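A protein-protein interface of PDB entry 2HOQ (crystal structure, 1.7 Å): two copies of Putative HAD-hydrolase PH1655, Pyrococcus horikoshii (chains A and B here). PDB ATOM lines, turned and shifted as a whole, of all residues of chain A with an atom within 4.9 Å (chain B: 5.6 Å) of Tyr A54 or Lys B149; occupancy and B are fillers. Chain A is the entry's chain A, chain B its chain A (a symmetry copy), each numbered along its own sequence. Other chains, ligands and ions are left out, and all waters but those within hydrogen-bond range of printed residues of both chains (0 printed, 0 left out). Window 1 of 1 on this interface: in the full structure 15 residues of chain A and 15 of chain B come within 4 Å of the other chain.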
ATOM      1  N   LEU A  50      12.309  20.449 -11.792  1.00  0.00           N
ATOM      2  CA  LEU A  50      11.024  20.318 -11.117  1.00  0.00           C
ATOM      3  C   LEU A  50      10.768  18.859 -10.758  1.00  0.00           C
ATOM      4  O   LEU A  50      10.244  18.550  -9.683  1.00  0.00           O
ATOM      5  CB  LEU A  50       9.904  20.841 -12.022  1.00  0.00           C
ATOM      6  CG  LEU A  50       8.512  20.992 -11.414  1.00  0.00           C
ATOM      7  CD1 LEU A  50       8.527  22.113 -10.394  1.00  0.00           C
ATOM      8  N   ILE A  51      11.151  17.959 -11.660  1.00  0.00           N
ATOM      9  CA  ILE A  51      10.957  16.531 -11.443  1.00  0.00           C
ATOM     10  C   ILE A  51      11.836  16.022 -10.303  1.00  0.00           C
ATOM     11  O   ILE A  51      11.427  15.153  -9.531  1.00  0.00           O
ATOM     12  CB  ILE A  51      11.269  15.735 -12.735  1.00  0.00           C
ATOM     13  CG1 ILE A  51      10.169  15.991 -13.766  1.00  0.00           C
ATOM     14  CG2 ILE A  51      11.390  14.245 -12.429  1.00  0.00           C
ATOM     15  CD1 ILE A  51      10.427  15.361 -15.119  1.00  0.00           C
ATOM     16  N   LYS A  52      13.041  16.570 -10.195  1.00  0.00           N
ATOM     17  CA  LYS A  52      13.958  16.160  -9.141  1.00  0.00           C
ATOM     18  C   LYS A  52      13.553  16.743  -7.789  1.00  0.00           C
ATOM     19  O   LYS A  52      13.892  16.197  -6.738  1.00  0.00           O
ATOM     20  CB  LYS A  52      15.381  16.590  -9.493  1.00  0.00           C
ATOM     21  CG  LYS A  52      15.904  15.946 -10.769  1.00  0.00           C
ATOM     22  N   GLU A  53      12.819  17.850  -7.821  1.00  0.00           N
ATOM     23  CA  GLU A  53      12.372  18.513  -6.600  1.00  0.00           C
ATOM     24  C   GLU A  53      11.041  17.977  -6.086  1.00  0.00           C
ATOM     25  O   GLU A  53      10.836  17.862  -4.876  1.00  0.00           O
ATOM     26  CB  GLU A  53      12.253  20.028  -6.837  1.00  0.00           C
ATOM     27  CG  GLU A  53      13.579  20.792  -6.781  1.00  0.00           C
ATOM     28  CD  GLU A  53      13.463  22.227  -7.283  1.00  0.00           C
ATOM     29  OE1 GLU A  53      12.401  22.851  -7.077  1.00  0.00           O
ATOM     30  OE2 GLU A  53      14.440  22.737  -7.873  1.00  0.00           O
ATOM     31  N   TYR A  54      10.146  17.637  -7.008  1.00  0.00           N
ATOM     32  CA  TYR A  54       8.818  17.142  -6.657  1.00  0.00           C
ATOM     33  C   TYR A  54       8.591  15.646  -6.859  1.00  0.00           C
ATOM     34  O   TYR A  54       7.575  15.108  -6.417  1.00  0.00           O
ATOM     35  CB  TYR A  54       7.758  17.935  -7.434  1.00  0.00           C
ATOM     36  CG  TYR A  54       7.500  19.326  -6.889  1.00  0.00           C
ATOM     37  CD1 TYR A  54       6.485  19.557  -5.958  1.00  0.00           C
ATOM     38  CD2 TYR A  54       8.282  20.412  -7.288  1.00  0.00           C
ATOM     39  CE1 TYR A  54       6.255  20.838  -5.436  1.00  0.00           C
ATOM     40  CE2 TYR A  54       8.062  21.690  -6.773  1.00  0.00           C
ATOM     41  CZ  TYR A  54       7.049  21.898  -5.851  1.00  0.00           C
ATOM     42  OH  TYR A  54       6.834  23.164  -5.347  1.00  0.00           O
ATOM     43  N   GLY A  55       9.519  14.970  -7.528  1.00  0.00           N
ATOM     44  CA  GLY A  55       9.359  13.540  -7.740  1.00  0.00           C
ATOM     45  C   GLY A  55       8.866  13.146  -9.120  1.00  0.00           C
ATOM     46  O   GLY A  55       8.145  13.895  -9.773  1.00  0.00           O
ATOM     47  N   SER A  56       9.248  11.948  -9.554  1.00  0.00           N
ATOM     48  CA  SER A  56       8.873  11.436 -10.865  1.00  0.00           C
ATOM     49  C   SER A  56       7.376  11.223 -11.072  1.00  0.00           C
ATOM     50  O   SER A  56       6.879  11.356 -12.190  1.00  0.00           O
ATOM     51  CB  SER A  56       9.609  10.121 -11.138  1.00  0.00           C
ATOM     52  N   PHE A  58       4.875  12.989  -9.509  1.00  0.00           N
ATOM     53  CA  PHE A  58       4.072  14.141  -9.103  1.00  0.00           C
ATOM     54  C   PHE A  58       3.077  14.349 -10.243  1.00  0.00           C
ATOM     55  O   PHE A  58       3.461  14.369 -11.413  1.00  0.00           O
ATOM     56  CB  PHE A  58       4.955  15.381  -8.941  1.00  0.00           C
ATOM     57  CG  PHE A  58       4.230  16.580  -8.403  1.00  0.00           C
ATOM     58  CD1 PHE A  58       3.731  16.584  -7.102  1.00  0.00           C
ATOM     59  CD2 PHE A  58       4.050  17.712  -9.193  1.00  0.00           C
ATOM     60  CE1 PHE A  58       3.067  17.698  -6.595  1.00  0.00           C
ATOM     61  CE2 PHE A  58       3.386  18.833  -8.697  1.00  0.00           C
ATOM     62  CZ  PHE A  58       2.894  18.828  -7.396  1.00  0.00           C
ATOM     63  N   HIS A  61       3.322  18.328 -12.808  1.00  0.00           N
ATOM     64  CA  HIS A  61       4.574  18.899 -13.312  1.00  0.00           C
ATOM     65  C   HIS A  61       4.345  20.090 -14.236  1.00  0.00           C
ATOM     66  O   HIS A  61       4.994  21.126 -14.098  1.00  0.00           O
ATOM     67  CB  HIS A  61       5.385  17.864 -14.093  1.00  0.00           C
ATOM     68  CG  HIS A  61       5.883  16.724 -13.265  1.00  0.00           C
ATOM     69  ND1 HIS A  61       6.617  16.903 -12.113  1.00  0.00           N
ATOM     70  CD2 HIS A  61       5.780  15.386 -13.442  1.00  0.00           C
ATOM     71  CE1 HIS A  61       6.945  15.723 -11.615  1.00  0.00           C
ATOM     72  NE2 HIS A  61       6.448  14.786 -12.402  1.00  0.00           N
ATOM     73  N   TYR A  64       2.959  23.155 -12.351  1.00  0.00           N
ATOM     74  CA  TYR A  64       4.025  23.751 -11.557  1.00  0.00           C
ATOM     75  C   TYR A  64       5.130  24.370 -12.404  1.00  0.00           C
ATOM     76  O   TYR A  64       5.823  25.276 -11.943  1.00  0.00           O
ATOM     77  CB  TYR A  64       4.607  22.725 -10.583  1.00  0.00           C
ATOM     78  CG  TYR A  64       3.789  22.579  -9.315  1.00  0.00           C
ATOM     79  CD1 TYR A  64       2.424  22.300  -9.373  1.00  0.00           C
ATOM     80  CD2 TYR A  64       4.380  22.720  -8.060  1.00  0.00           C
ATOM     81  CE1 TYR A  64       1.665  22.166  -8.210  1.00  0.00           C
ATOM     82  CE2 TYR A  64       3.630  22.587  -6.889  1.00  0.00           C
ATOM     83  CZ  TYR A  64       2.275  22.311  -6.974  1.00  0.00           C
ATOM     84  OH  TYR A  64       1.522  22.181  -5.829  1.00  0.00           O
ATOM     85  N   ASP B 118       7.941  24.621   2.700  1.00  0.00           N
ATOM     86  CA  ASP B 118       7.562  23.861   1.510  1.00  0.00           C
ATOM     87  C   ASP B 118       6.279  23.117   1.857  1.00  0.00           C
ATOM     88  O   ASP B 118       5.884  23.056   3.026  1.00  0.00           O
ATOM     89  CB  ASP B 118       8.611  22.791   1.160  1.00  0.00           C
ATOM     90  CG  ASP B 118       9.982  23.367   0.859  1.00  0.00           C
ATOM     91  OD1 ASP B 118      10.090  24.266   0.007  1.00  0.00           O
ATOM     92  OD2 ASP B 118      10.961  22.898   1.477  1.00  0.00           O
ATOM     93  N   GLY B 119       5.638  22.556   0.842  1.00  0.00           N
ATOM     94  CA  GLY B 119       4.445  21.764   1.079  1.00  0.00           C
ATOM     95  C   GLY B 119       3.115  22.319   0.636  1.00  0.00           C
ATOM     96  O   GLY B 119       2.992  23.484   0.273  1.00  0.00           O
ATOM     97  N   SER B 143       6.646  27.694  -0.770  1.00  0.00           N
ATOM     98  CA  SER B 143       7.326  27.422  -2.029  1.00  0.00           C
ATOM     99  C   SER B 143       6.470  26.853  -3.153  1.00  0.00           C
ATOM    100  O   SER B 143       6.688  27.176  -4.317  1.00  0.00           O
ATOM    101  CB  SER B 143       8.519  26.494  -1.779  1.00  0.00           C
ATOM    102  OG  SER B 143       8.080  25.201  -1.400  1.00  0.00           O
ATOM    103  N   ASP B 144       5.498  26.012  -2.814  1.00  0.00           N
ATOM    104  CA  ASP B 144       4.645  25.414  -3.833  1.00  0.00           C
ATOM    105  C   ASP B 144       3.920  26.443  -4.697  1.00  0.00           C
ATOM    106  O   ASP B 144       3.662  26.190  -5.875  1.00  0.00           O
ATOM    107  CB  ASP B 144       3.650  24.455  -3.180  1.00  0.00           C
ATOM    108  CG  ASP B 144       4.329  23.223  -2.605  1.00  0.00           C
ATOM    109  OD1 ASP B 144       5.274  23.387  -1.802  1.00  0.00           O
ATOM    110  OD2 ASP B 144       3.927  22.093  -2.957  1.00  0.00           O
ATOM    111  N   GLY B 147       6.229  27.120  -7.514  1.00  0.00           N
ATOM    112  CA  GLY B 147       6.700  26.018  -8.341  1.00  0.00           C
ATOM    113  C   GLY B 147       8.140  25.593  -8.105  1.00  0.00           C
ATOM    114  O   GLY B 147       8.796  25.057  -9.004  1.00  0.00           O
ATOM    115  N   VAL B 148       8.637  25.829  -6.895  1.00  0.00           N
ATOM    116  CA  VAL B 148      10.005  25.456  -6.539  1.00  0.00           C
ATOM    117  C   VAL B 148      10.014  24.884  -5.128  1.00  0.00           C
ATOM    118  O   VAL B 148       9.018  24.941  -4.419  1.00  0.00           O
ATOM    119  CB  VAL B 148      10.977  26.683  -6.530  1.00  0.00           C
ATOM    120  CG1 VAL B 148      10.990  27.370  -7.895  1.00  0.00           C
ATOM    121  CG2 VAL B 148      10.570  27.667  -5.432  1.00  0.00           C
ATOM    122  N   LYS B 149      11.144  24.309  -4.736  1.00  0.00           N
ATOM    123  CA  LYS B 149      11.297  23.798  -3.380  1.00  0.00           C
ATOM    124  C   LYS B 149      12.530  24.492  -2.814  1.00  0.00           C
ATOM    125  O   LYS B 149      13.435  24.836  -3.572  1.00  0.00           O
ATOM    126  CB  LYS B 149      11.542  22.287  -3.383  1.00  0.00           C
ATOM    127  CG  LYS B 149      10.319  21.435  -3.679  1.00  0.00           C
ATOM    128  CD  LYS B 149       9.351  21.430  -2.515  1.00  0.00           C
ATOM    129  CE  LYS B 149       8.330  20.305  -2.654  1.00  0.00           C
ATOM    130  N   LYS B 150      12.561  24.727  -1.505  1.00  0.00           N
ATOM    131  CA  LYS B 150      13.746  25.340  -0.904  1.00  0.00           C
ATOM    132  C   LYS B 150      14.843  24.320  -1.210  1.00  0.00           C
ATOM    133  O   LYS B 150      14.566  23.125  -1.292  1.00  0.00           O
ATOM    134  CB  LYS B 150      13.571  25.505   0.614  1.00  0.00           C
ATOM    135  CG  LYS B 150      12.529  26.551   1.005  1.00  0.00           C
ATOM    136  CD  LYS B 150      12.516  26.844   2.517  1.00  0.00           C
ATOM    137  CE  LYS B 150      12.010  25.673   3.332  1.00  0.00           C
ATOM    138  NZ  LYS B 150      11.821  26.024   4.776  1.00  0.00           N
ATOM    139  N   PRO B 151      16.107  24.756  -1.332  1.00  0.00           N
ATOM    140  CA  PRO B 151      16.675  26.102  -1.209  1.00  0.00           C
ATOM    141  C   PRO B 151      16.655  26.990  -2.455  1.00  0.00           C
ATOM    142  O   PRO B 151      17.475  27.904  -2.567  1.00  0.00           O
ATOM    143  CB  PRO B 151      18.101  25.813  -0.763  1.00  0.00           C
ATOM    144  CG  PRO B 151      18.439  24.624  -1.612  1.00  0.00           C
ATOM    145  CD  PRO B 151      17.187  23.756  -1.456  1.00  0.00           C
ATOM    146  N   HIS B 152      15.740  26.746  -3.388  1.00  0.00           N
ATOM    147  CA  HIS B 152      15.707  27.578  -4.593  1.00  0.00           C
ATOM    148  C   HIS B 152      15.628  29.063  -4.205  1.00  0.00           C
ATOM    149  O   HIS B 152      14.781  29.462  -3.410  1.00  0.00           O
ATOM    150  CB  HIS B 152      14.513  27.198  -5.473  1.00  0.00           C
ATOM    151  CG  HIS B 152      14.568  27.799  -6.841  1.00  0.00           C
ATOM    152  ND1 HIS B 152      14.729  27.045  -7.984  1.00  0.00           N
ATOM    153  CD2 HIS B 152      14.498  29.088  -7.248  1.00  0.00           C
ATOM    154  CE1 HIS B 152      14.755  27.844  -9.036  1.00  0.00           C
ATOM    155  NE2 HIS B 152      14.617  29.089  -8.616  1.00  0.00           N
ATOM    156  N   ILE B 155      12.092  31.458  -3.902  1.00  0.00           N
ATOM    157  CA  ILE B 155      11.198  31.558  -2.756  1.00  0.00           C
ATOM    158  C   ILE B 155      11.731  32.491  -1.669  1.00  0.00           C
ATOM    159  O   ILE B 155      10.953  33.183  -1.010  1.00  0.00           O
ATOM    160  CB  ILE B 155      10.871  30.152  -2.185  1.00  0.00           C
ATOM    161  CG1 ILE B 155       9.640  30.237  -1.283  1.00  0.00           C
ATOM    162  CG2 ILE B 155      12.061  29.590  -1.433  1.00  0.00           C
ATOM    163  CD1 ILE B 155       8.411  30.800  -1.988  1.00  0.00           C
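OE1 of Glu A53 sits at hydrogen-bond distance from N of Lys B149. The side-chain hydroxyl (OH) of Tyr A54 lies within hydrogen-bond range of the backbone carbonyl oxygen (O) of Val B148 (3.0 Å).
N of Gly B119 sits at hydrogen-bond distance from OD1 of Asp B144 (2.8 Å). OD1 of Asp B144 is in hydrogen-bond range of OG of Ser B143. The side-chain hydroxyl of Ser B143 lies close to the backbone carbonyl oxygen of Val B148.
O of Gly B147 touches CD1 of Leu A50, 3.3 Å away. Glu A53 touches Val B148 (OE1 to CA, 3.6 Å). OH of Tyr A54 touches CA of Asp B144 (3.5 Å). Gly B147 touches Tyr A54. Tyr A54 touches Lys B149. Tyr A64 touches Asp B144 (CE2 to O, 3.7 Å). O of Tyr A64 touches CA of Gly B147, 3.8 Å away.
Tyr A54 touches four residues of chain B. Lys B149 touches two residues of chain A. Of the printed residues of chain A, Gly B147 touches Leu A50 (3.3 Å), Tyr A54 (3.9 Å) and Tyr A64 (3.8 Å). Printed residues of chain A within 4 Å of Val B148: Glu A53 (3.6 Å) and Tyr A54 (3.0 Å). Printed residues of chain B within 4 Å of Leu A50: Gly B147 (3.3 Å). Gly B119 touches none of the printed residues of chain A. The nearest printed residue of chain A that does not touch Lys B149 is Leu A50 (6.6 Å). The nearest printed residue of chain B that does not touch Leu A50 is Val B148 (5.1 Å).
Hydrophobic or aromatic side chains of chain A within 4 Å of the printed part of chain B: Leu A50, Tyr A54 and Tyr A64. Of the 11 printed residues of chain B, 4 touch a printed residue of chain A. Printed residues of chain B that touch a printed residue of chain A: Asp B144, Gly B147, Val B148 and Lys B149. Along chain B the printed residues that touch a printed residue of chain A span positions 144 to 149. Among the printed residues, 9 pairs touch across the chains.
No position is printed for both chains. Of the 9 pairs that touch across the chains among the printed residues, none has its exchanged pair printed and touching as well.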
